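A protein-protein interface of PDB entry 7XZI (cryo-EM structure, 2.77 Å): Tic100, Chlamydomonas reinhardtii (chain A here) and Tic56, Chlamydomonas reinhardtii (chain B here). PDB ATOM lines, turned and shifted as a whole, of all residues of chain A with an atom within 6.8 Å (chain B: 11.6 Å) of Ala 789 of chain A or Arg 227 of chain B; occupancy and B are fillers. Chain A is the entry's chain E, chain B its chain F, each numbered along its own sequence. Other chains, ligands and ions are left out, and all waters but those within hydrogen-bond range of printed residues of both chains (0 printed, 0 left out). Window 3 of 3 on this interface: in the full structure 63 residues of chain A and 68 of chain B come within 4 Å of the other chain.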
ATOM      1  N   GLY A 775      25.996 -19.136   4.509  1.00  0.00           N
ATOM      2  CA  GLY A 775      25.013 -20.056   5.063  1.00  0.00           C
ATOM      3  C   GLY A 775      25.480 -21.493   5.139  1.00  0.00           C
ATOM      4  O   GLY A 775      24.708 -22.411   4.834  1.00  0.00           O
ATOM      5  N   LYS A 777      26.884 -22.643   8.096  1.00  0.00           N
ATOM      6  CA  LYS A 777      27.123 -22.823   9.522  1.00  0.00           C
ATOM      7  C   LYS A 777      26.642 -24.172  10.034  1.00  0.00           C
ATOM      8  O   LYS A 777      26.970 -24.534  11.169  1.00  0.00           O
ATOM      9  CB  LYS A 777      26.452 -21.702  10.316  1.00  0.00           C
ATOM     10  CG  LYS A 777      26.817 -20.307   9.840  1.00  0.00           C
ATOM     11  CD  LYS A 777      26.287 -19.238  10.781  1.00  0.00           C
ATOM     12  CE  LYS A 777      26.510 -17.849  10.205  1.00  0.00           C
ATOM     13  NZ  LYS A 777      27.939 -17.617   9.858  1.00  0.00           N
ATOM     14  N   PHE A 778      25.876 -24.919   9.236  1.00  0.00           N
ATOM     15  CA  PHE A 778      25.482 -26.267   9.623  1.00  0.00           C
ATOM     16  C   PHE A 778      26.656 -27.236   9.631  1.00  0.00           C
ATOM     17  O   PHE A 778      26.524 -28.336  10.175  1.00  0.00           O
ATOM     18  CB  PHE A 778      24.386 -26.786   8.689  1.00  0.00           C
ATOM     19  CG  PHE A 778      24.853 -27.042   7.283  1.00  0.00           C
ATOM     20  CD1 PHE A 778      24.918 -26.010   6.362  1.00  0.00           C
ATOM     21  CD2 PHE A 778      25.217 -28.316   6.880  1.00  0.00           C
ATOM     22  CE1 PHE A 778      25.343 -26.244   5.068  1.00  0.00           C
ATOM     23  CE2 PHE A 778      25.643 -28.555   5.590  1.00  0.00           C
ATOM     24  CZ  PHE A 778      25.706 -27.518   4.682  1.00  0.00           C
ATOM     25  N   GLY A 785      26.105 -25.751  15.006  1.00  0.00           N
ATOM     26  CA  GLY A 785      25.600 -26.381  13.797  1.00  0.00           C
ATOM     27  C   GLY A 785      24.137 -26.771  13.899  1.00  0.00           C
ATOM     28  O   GLY A 785      23.392 -26.679  12.920  1.00  0.00           O
ATOM     29  N   LEU A 786      23.707 -27.216  15.081  1.00  0.00           N
ATOM     30  CA  LEU A 786      22.323 -27.647  15.253  1.00  0.00           C
ATOM     31  C   LEU A 786      21.352 -26.481  15.122  1.00  0.00           C
ATOM     32  O   LEU A 786      20.180 -26.675  14.781  1.00  0.00           O
ATOM     33  CB  LEU A 786      22.152 -28.336  16.606  1.00  0.00           C
ATOM     34  CG  LEU A 786      22.968 -29.607  16.833  1.00  0.00           C
ATOM     35  CD1 LEU A 786      22.547 -30.287  18.122  1.00  0.00           C
ATOM     36  CD2 LEU A 786      22.817 -30.551  15.652  1.00  0.00           C
ATOM     37  N   CYS A 787      21.817 -25.259  15.396  1.00  0.00           N
ATOM     38  CA  CYS A 787      20.940 -24.096  15.307  1.00  0.00           C
ATOM     39  C   CYS A 787      20.482 -23.834  13.879  1.00  0.00           C
ATOM     40  O   CYS A 787      19.369 -23.341  13.663  1.00  0.00           O
ATOM     41  CB  CYS A 787      21.648 -22.866  15.873  1.00  0.00           C
ATOM     42  SG  CYS A 787      22.129 -23.029  17.606  1.00  0.00           S
ATOM     43  N   HIS A 788      21.317 -24.152  12.895  1.00  0.00           N
ATOM     44  CA  HIS A 788      21.014 -23.905  11.494  1.00  0.00           C
ATOM     45  C   HIS A 788      20.567 -25.193  10.808  1.00  0.00           C
ATOM     46  O   HIS A 788      20.705 -26.295  11.341  1.00  0.00           O
ATOM     47  CB  HIS A 788      22.229 -23.304  10.787  1.00  0.00           C
ATOM     48  CG  HIS A 788      22.720 -22.038  11.416  1.00  0.00           C
ATOM     49  ND1 HIS A 788      22.356 -20.789  10.959  1.00  0.00           N
ATOM     50  CD2 HIS A 788      23.531 -21.827  12.479  1.00  0.00           C
ATOM     51  CE1 HIS A 788      22.929 -19.865  11.708  1.00  0.00           C
ATOM     52  NE2 HIS A 788      23.647 -20.468  12.638  1.00  0.00           N
ATOM     53  N   ALA A 789      20.025 -25.036   9.604  1.00  0.00           N
ATOM     54  CA  ALA A 789      19.417 -26.130   8.863  1.00  0.00           C
ATOM     55  C   ALA A 789      20.274 -26.519   7.665  1.00  0.00           C
ATOM     56  O   ALA A 789      21.057 -25.723   7.143  1.00  0.00           O
ATOM     57  CB  ALA A 789      18.008 -25.753   8.392  1.00  0.00           C
ATOM     58  N   VAL A 790      20.107 -27.766   7.235  1.00  0.00           N
ATOM     59  CA  VAL A 790      20.839 -28.316   6.098  1.00  0.00           C
ATOM     60  C   VAL A 790      20.176 -27.856   4.803  1.00  0.00           C
ATOM     61  O   VAL A 790      18.974 -27.552   4.798  1.00  0.00           O
ATOM     62  CB  VAL A 790      20.909 -29.849   6.185  1.00  0.00           C
ATOM     63  CG1 VAL A 790      21.769 -30.264   7.369  1.00  0.00           C
ATOM     64  CG2 VAL A 790      19.514 -30.431   6.312  1.00  0.00           C
ATOM     65  N   PRO A 791      20.906 -27.787   3.688  1.00  0.00           N
ATOM     66  CA  PRO A 791      20.343 -27.238   2.448  1.00  0.00           C
ATOM     67  C   PRO A 791      19.361 -28.148   1.724  1.00  0.00           C
ATOM     68  O   PRO A 791      18.989 -27.834   0.590  1.00  0.00           O
ATOM     69  CB  PRO A 791      21.593 -27.003   1.579  1.00  0.00           C
ATOM     70  CG  PRO A 791      22.753 -27.036   2.526  1.00  0.00           C
ATOM     71  CD  PRO A 791      22.355 -28.013   3.576  1.00  0.00           C
ATOM     72  N   ASP A 792      18.935 -29.257   2.335  1.00  0.00           N
ATOM     73  CA  ASP A 792      17.919 -30.146   1.761  1.00  0.00           C
ATOM     74  C   ASP A 792      18.374 -30.740   0.428  1.00  0.00           C
ATOM     75  O   ASP A 792      17.754 -30.521  -0.615  1.00  0.00           O
ATOM     76  CB  ASP A 792      16.574 -29.427   1.607  1.00  0.00           C
ATOM     77  CG  ASP A 792      15.429 -30.380   1.292  1.00  0.00           C
ATOM     78  OD1 ASP A 792      15.632 -31.609   1.359  1.00  0.00           O
ATOM     79  OD2 ASP A 792      14.322 -29.895   0.976  1.00  0.00           O
ATOM     80  N   ARG A 797      22.912 -35.151   2.351  1.00  0.00           N
ATOM     81  CA  ARG A 797      22.463 -35.822   3.567  1.00  0.00           C
ATOM     82  C   ARG A 797      23.104 -37.196   3.712  1.00  0.00           C
ATOM     83  O   ARG A 797      23.503 -37.586   4.814  1.00  0.00           O
ATOM     84  CB  ARG A 797      20.940 -35.937   3.571  1.00  0.00           C
ATOM     85  CG  ARG A 797      20.216 -34.603   3.604  1.00  0.00           C
ATOM     86  CD  ARG A 797      18.709 -34.792   3.594  1.00  0.00           C
ATOM     87  NE  ARG A 797      17.999 -33.521   3.612  1.00  0.00           N
ATOM     88  CZ  ARG A 797      17.594 -32.904   4.716  1.00  0.00           C
ATOM     89  NH1 ARG A 797      17.816 -33.416   5.915  1.00  0.00           N
ATOM     90  NH2 ARG A 797      16.946 -31.748   4.612  1.00  0.00           N
ATOM     91  N   ARG B 150      31.775 -31.251  10.275  1.00  0.00           N
ATOM     92  CA  ARG B 150      30.792 -32.284   9.964  1.00  0.00           C
ATOM     93  C   ARG B 150      30.984 -32.848   8.564  1.00  0.00           C
ATOM     94  O   ARG B 150      30.542 -33.969   8.283  1.00  0.00           O
ATOM     95  CB  ARG B 150      29.375 -31.729  10.110  1.00  0.00           C
ATOM     96  CG  ARG B 150      29.006 -31.306  11.521  1.00  0.00           C
ATOM     97  CD  ARG B 150      27.524 -30.985  11.618  1.00  0.00           C
ATOM     98  NE  ARG B 150      27.150 -30.480  12.931  1.00  0.00           N
ATOM     99  CZ  ARG B 150      26.732 -31.241  13.937  1.00  0.00           C
ATOM    100  NH1 ARG B 150      26.642 -32.555  13.817  1.00  0.00           N
ATOM    101  NH2 ARG B 150      26.396 -30.667  15.088  1.00  0.00           N
ATOM    102  N   MET B 151      31.623 -32.096   7.673  1.00  0.00           N
ATOM    103  CA  MET B 151      31.872 -32.540   6.311  1.00  0.00           C
ATOM    104  C   MET B 151      33.216 -33.242   6.157  1.00  0.00           C
ATOM    105  O   MET B 151      33.632 -33.509   5.025  1.00  0.00           O
ATOM    106  CB  MET B 151      31.787 -31.357   5.344  1.00  0.00           C
ATOM    107  CG  MET B 151      30.407 -30.727   5.262  1.00  0.00           C
ATOM    108  SD  MET B 151      29.130 -31.920   4.816  1.00  0.00           S
ATOM    109  CE  MET B 151      29.730 -32.481   3.224  1.00  0.00           C
ATOM    110  N   PRO B 218      17.937 -20.290  23.132  1.00  0.00           N
ATOM    111  CA  PRO B 218      16.719 -19.697  22.555  1.00  0.00           C
ATOM    112  C   PRO B 218      16.653 -19.820  21.044  1.00  0.00           C
ATOM    113  O   PRO B 218      15.563 -20.005  20.491  1.00  0.00           O
ATOM    114  CB  PRO B 218      16.791 -18.233  23.010  1.00  0.00           C
ATOM    115  CG  PRO B 218      18.229 -17.987  23.258  1.00  0.00           C
ATOM    116  CD  PRO B 218      18.750 -19.271  23.823  1.00  0.00           C
ATOM    117  N   SER B 219      17.794 -19.726  20.359  1.00  0.00           N
ATOM    118  CA  SER B 219      17.797 -19.886  18.907  1.00  0.00           C
ATOM    119  C   SER B 219      17.423 -21.309  18.509  1.00  0.00           C
ATOM    120  O   SER B 219      16.705 -21.516  17.526  1.00  0.00           O
ATOM    121  CB  SER B 219      19.164 -19.507  18.340  1.00  0.00           C
ATOM    122  OG  SER B 219      19.462 -18.146  18.599  1.00  0.00           O
ATOM    123  N   LEU B 220      17.904 -22.300  19.262  1.00  0.00           N
ATOM    124  CA  LEU B 220      17.521 -23.683  19.004  1.00  0.00           C
ATOM    125  C   LEU B 220      16.030 -23.889  19.236  1.00  0.00           C
ATOM    126  O   LEU B 220      15.358 -24.566  18.449  1.00  0.00           O
ATOM    127  CB  LEU B 220      18.340 -24.630  19.881  1.00  0.00           C
ATOM    128  CG  LEU B 220      18.080 -26.126  19.695  1.00  0.00           C
ATOM    129  CD1 LEU B 220      18.362 -26.539  18.260  1.00  0.00           C
ATOM    130  CD2 LEU B 220      18.915 -26.947  20.668  1.00  0.00           C
ATOM    131  N   ASN B 221      15.492 -23.307  20.309  1.00  0.00           N
ATOM    132  CA  ASN B 221      14.054 -23.406  20.551  1.00  0.00           C
ATOM    133  C   ASN B 221      13.264 -22.764  19.415  1.00  0.00           C
ATOM    134  O   ASN B 221      12.265 -23.321  18.943  1.00  0.00           O
ATOM    135  CB  ASN B 221      13.697 -22.761  21.890  1.00  0.00           C
ATOM    136  CG  ASN B 221      14.298 -23.496  23.070  1.00  0.00           C
ATOM    137  OD1 ASN B 221      14.590 -24.689  22.991  1.00  0.00           O
ATOM    138  ND2 ASN B 221      14.482 -22.786  24.177  1.00  0.00           N
ATOM    139  N   ARG B 222      13.708 -21.590  18.958  1.00  0.00           N
ATOM    140  CA  ARG B 222      13.012 -20.891  17.883  1.00  0.00           C
ATOM    141  C   ARG B 222      13.062 -21.680  16.581  1.00  0.00           C
ATOM    142  O   ARG B 222      12.063 -21.758  15.858  1.00  0.00           O
ATOM    143  CB  ARG B 222      13.613 -19.498  17.692  1.00  0.00           C
ATOM    144  CG  ARG B 222      12.961 -18.682  16.588  1.00  0.00           C
ATOM    145  CD  ARG B 222      13.557 -17.283  16.489  1.00  0.00           C
ATOM    146  NE  ARG B 222      13.276 -16.473  17.667  1.00  0.00           N
ATOM    147  CZ  ARG B 222      14.134 -16.268  18.661  1.00  0.00           C
ATOM    148  NH1 ARG B 222      15.346 -16.797  18.649  1.00  0.00           N
ATOM    149  NH2 ARG B 222      13.764 -15.514  19.691  1.00  0.00           N
ATOM    150  N   ILE B 223      14.217 -22.267  16.257  1.00  0.00           N
ATOM    151  CA  ILE B 223      14.325 -23.017  15.010  1.00  0.00           C
ATOM    152  C   ILE B 223      13.537 -24.321  15.094  1.00  0.00           C
ATOM    153  O   ILE B 223      13.003 -24.793  14.082  1.00  0.00           O
ATOM    154  CB  ILE B 223      15.803 -23.252  14.637  1.00  0.00           C
ATOM    155  CG1 ILE B 223      15.920 -23.708  13.181  1.00  0.00           C
ATOM    156  CG2 ILE B 223      16.459 -24.267  15.555  1.00  0.00           C
ATOM    157  CD1 ILE B 223      15.448 -22.676  12.184  1.00  0.00           C
ATOM    158  N   ARG B 224      13.448 -24.928  16.281  1.00  0.00           N
ATOM    159  CA  ARG B 224      12.597 -26.102  16.442  1.00  0.00           C
ATOM    160  C   ARG B 224      11.126 -25.745  16.270  1.00  0.00           C
ATOM    161  O   ARG B 224      10.369 -26.497  15.646  1.00  0.00           O
ATOM    162  CB  ARG B 224      12.837 -26.745  17.807  1.00  0.00           C
ATOM    163  CG  ARG B 224      14.147 -27.501  17.913  1.00  0.00           C
ATOM    164  CD  ARG B 224      14.375 -28.013  19.322  1.00  0.00           C
ATOM    165  NE  ARG B 224      15.581 -28.822  19.414  1.00  0.00           N
ATOM    166  CZ  ARG B 224      16.064 -29.323  20.547  1.00  0.00           C
ATOM    167  NH1 ARG B 224      15.470 -29.104  21.708  1.00  0.00           N
ATOM    168  NH2 ARG B 224      17.170 -30.058  20.510  1.00  0.00           N
ATOM    169  N   GLU B 225      10.703 -24.605  16.820  1.00  0.00           N
ATOM    170  CA  GLU B 225       9.303 -24.208  16.705  1.00  0.00           C
ATOM    171  C   GLU B 225       8.947 -23.771  15.289  1.00  0.00           C
ATOM    172  O   GLU B 225       7.819 -23.999  14.838  1.00  0.00           O
ATOM    173  CB  GLU B 225       8.994 -23.087  17.698  1.00  0.00           C
ATOM    174  N   GLN B 226       9.885 -23.143  14.578  1.00  0.00           N
ATOM    175  CA  GLN B 226       9.582 -22.574  13.268  1.00  0.00           C
ATOM    176  C   GLN B 226       9.434 -23.646  12.193  1.00  0.00           C
ATOM    177  O   GLN B 226       8.507 -23.585  11.378  1.00  0.00           O
ATOM    178  CB  GLN B 226      10.670 -21.575  12.872  1.00  0.00           C
ATOM    179  CG  GLN B 226      10.481 -20.957  11.496  1.00  0.00           C
ATOM    180  CD  GLN B 226      11.624 -20.038  11.111  1.00  0.00           C
ATOM    181  OE1 GLN B 226      12.592 -19.887  11.856  1.00  0.00           O
ATOM    182  NE2 GLN B 226      11.517 -19.418   9.942  1.00  0.00           N
ATOM    183  N   ARG B 227      10.327 -24.632  12.175  1.00  0.00           N
ATOM    184  CA  ARG B 227      10.371 -25.634  11.118  1.00  0.00           C
ATOM    185  C   ARG B 227      10.017 -26.997  11.693  1.00  0.00           C
ATOM    186  O   ARG B 227      10.599 -27.425  12.695  1.00  0.00           O
ATOM    187  CB  ARG B 227      11.753 -25.668  10.457  1.00  0.00           C
ATOM    188  CG  ARG B 227      12.185 -24.322   9.891  1.00  0.00           C
ATOM    189  CD  ARG B 227      13.646 -24.313   9.462  1.00  0.00           C
ATOM    190  NE  ARG B 227      13.866 -24.997   8.196  1.00  0.00           N
ATOM    191  CZ  ARG B 227      14.392 -26.212   8.078  1.00  0.00           C
ATOM    192  NH1 ARG B 227      14.757 -26.913   9.139  1.00  0.00           N
ATOM    193  NH2 ARG B 227      14.559 -26.730   6.866  1.00  0.00           N
ATOM    194  N   LYS B 228       9.063 -27.675  11.052  1.00  0.00           N
ATOM    195  CA  LYS B 228       8.616 -28.989  11.495  1.00  0.00           C
ATOM    196  C   LYS B 228       9.584 -30.105  11.127  1.00  0.00           C
ATOM    197  O   LYS B 228       9.402 -31.236  11.593  1.00  0.00           O
ATOM    198  CB  LYS B 228       7.228 -29.292  10.918  1.00  0.00           C
ATOM    199  CG  LYS B 228       7.065 -28.969   9.432  1.00  0.00           C
ATOM    200  CD  LYS B 228       7.588 -30.087   8.538  1.00  0.00           C
ATOM    201  CE  LYS B 228       7.539 -29.704   7.069  1.00  0.00           C
ATOM    202  NZ  LYS B 228       8.127 -30.766   6.205  1.00  0.00           N
ATOM    203  N   GLU B 229      10.596 -29.822  10.302  1.00  0.00           N
ATOM    204  CA  GLU B 229      11.542 -30.854   9.894  1.00  0.00           C
ATOM    205  C   GLU B 229      12.342 -31.400  11.069  1.00  0.00           C
ATOM    206  O   GLU B 229      12.901 -32.498  10.967  1.00  0.00           O
ATOM    207  CB  GLU B 229      12.483 -30.303   8.821  1.00  0.00           C
ATOM    208  CG  GLU B 229      11.766 -29.755   7.595  1.00  0.00           C
ATOM    209  CD  GLU B 229      12.726 -29.223   6.549  1.00  0.00           C
ATOM    210  OE1 GLU B 229      13.942 -29.472   6.677  1.00  0.00           O
ATOM    211  OE2 GLU B 229      12.265 -28.551   5.602  1.00  0.00           O
ATOM    212  N   HIS B 230      12.413 -30.663  12.175  1.00  0.00           N
ATOM    213  CA  HIS B 230      13.022 -31.154  13.407  1.00  0.00           C
ATOM    214  C   HIS B 230      11.979 -31.974  14.158  1.00  0.00           C
ATOM    215  O   HIS B 230      11.093 -31.415  14.811  1.00  0.00           O
ATOM    216  CB  HIS B 230      13.530 -29.996  14.262  1.00  0.00           C
ATOM    217  CG  HIS B 230      14.562 -29.149  13.586  1.00  0.00           C
ATOM    218  ND1 HIS B 230      15.909 -29.258  13.857  1.00  0.00           N
ATOM    219  CD2 HIS B 230      14.444 -28.175  12.652  1.00  0.00           C
ATOM    220  CE1 HIS B 230      16.577 -28.390  13.119  1.00  0.00           C
ATOM    221  NE2 HIS B 230      15.711 -27.720  12.379  1.00  0.00           N
ATOM    222  N   ARG B 231      12.085 -33.298  14.066  1.00  0.00           N
ATOM    223  CA  ARG B 231      11.102 -34.189  14.676  1.00  0.00           C
ATOM    224  C   ARG B 231      11.201 -34.084  16.192  1.00  0.00           C
ATOM    225  O   ARG B 231      12.282 -34.255  16.764  1.00  0.00           O
ATOM    226  N   ASP B 232      10.072 -33.797  16.845  1.00  0.00           N
ATOM    227  CA  ASP B 232      10.031 -33.681  18.304  1.00  0.00           C
ATOM    228  C   ASP B 232      10.504 -34.936  19.028  1.00  0.00           C
ATOM    229  O   ASP B 232      11.286 -34.807  19.979  1.00  0.00           O
ATOM    230  CB  ASP B 232       8.602 -33.321  18.740  1.00  0.00           C
ATOM    231  N   PRO B 233      10.078 -36.146  18.655  1.00  0.00           N
ATOM    232  CA  PRO B 233      10.577 -37.338  19.362  1.00  0.00           C
ATOM    233  C   PRO B 233      12.081 -37.525  19.269  1.00  0.00           C
ATOM    234  O   PRO B 233      12.698 -38.019  20.222  1.00  0.00           O
ATOM    235  N   GLN B 234      12.690 -37.146  18.150  1.00  0.00           N
ATOM    236  CA  GLN B 234      14.126 -37.312  17.929  1.00  0.00           C
ATOM    237  C   GLN B 234      14.765 -35.926  17.871  1.00  0.00           C
ATOM    238  O   GLN B 234      14.903 -35.333  16.800  1.00  0.00           O
ATOM    239  CB  GLN B 234      14.394 -38.107  16.654  1.00  0.00           C
ATOM    240  CG  GLN B 234      13.782 -39.497  16.651  1.00  0.00           C
ATOM    241  N   GLU B 235      15.161 -35.415  19.034  1.00  0.00           N
ATOM    242  CA  GLU B 235      15.812 -34.117  19.150  1.00  0.00           C
ATOM    243  C   GLU B 235      17.141 -34.283  19.870  1.00  0.00           C
ATOM    244  O   GLU B 235      17.213 -34.961  20.901  1.00  0.00           O
ATOM    245  CB  GLU B 235      14.925 -33.118  19.897  1.00  0.00           C
ATOM    246  N   GLN B 239      23.133 -28.857  22.908  1.00  0.00           N
ATOM    247  CA  GLN B 239      23.154 -27.527  23.510  1.00  0.00           C
ATOM    248  C   GLN B 239      23.128 -27.601  25.032  1.00  0.00           C
ATOM    249  O   GLN B 239      23.712 -26.748  25.711  1.00  0.00           O
ATOM    250  CB  GLN B 239      21.975 -26.698  22.999  1.00  0.00           C
ATOM    251  CG  GLN B 239      22.348 -25.610  22.003  1.00  0.00           C
ATOM    252  CD  GLN B 239      22.610 -26.144  20.608  1.00  0.00           C
ATOM    253  OE1 GLN B 239      22.558 -27.350  20.370  1.00  0.00           O
ATOM    254  NE2 GLN B 239      22.888 -25.242  19.674  1.00  0.00           N
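Of the 12 printed residues of chain A, 4 touch a printed residue of chain B. Along chain A the printed residues that touch a printed residue of chain B span positions 778 to 789. Hydrophobic or aromatic side chains of chain B within 4 Å of the printed part of chain A: Leu 220 and Ile 223.
Phe 778 of chain A touches Arg 150 of chain B (O to CD, 3.2 Å). Arg 150 of chain B touches Leu 786 of chain A (NH2 to CD2, 3.6 Å). Leu 220 of chain B touches Leu 786 of chain A (CD1 to O, 3.9 Å). OE1 of Gln 239 of chain B touches CD1 of Leu 786 of chain A, 3.7 Å away. Cys 787 of chain A touches Ile 223 of chain B (O to CG1, 3.5 Å). Ala 789 of chain A touches Arg 227 of chain B.
SG of Cys 787 of chain A is in hydrogen-bond range of NE2 of Gln 239 of chain B (3.1 Å).
Ala 789 of chain A touches just one residue of chain B: Arg 227 (3.5 Å). No residue of chain B comes within 4 Å of Pro 791 of chain A. Ser 219 of chain B touches none of the printed residues of chain A. Printed residues of chain A within 4 Å of Ile 223 of chain B: Cys 787. Arg 227 of chain B touches just one residue of chain A: Ala 789. Of the printed residues of chain A, Gln 239 of chain B touches Leu 786 (3.7 Å) and Cys 787 (3.1 Å). The nearest residue of chain B that does not touch Ala 789 of chain A is His 230 of chain B (5.0 Å). The nearest printed residue of chain A that does not touch Leu 220 of chain B is Cys 787 of chain A (4.6 Å).
NH1 of Arg 227 of chain B lies within hydrogen-bond range of NE2 of His 230 of chain B. OE1 of Glu 229 of chain B lies within salt-bridge range of NH2 of Arg 227 of chain B.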
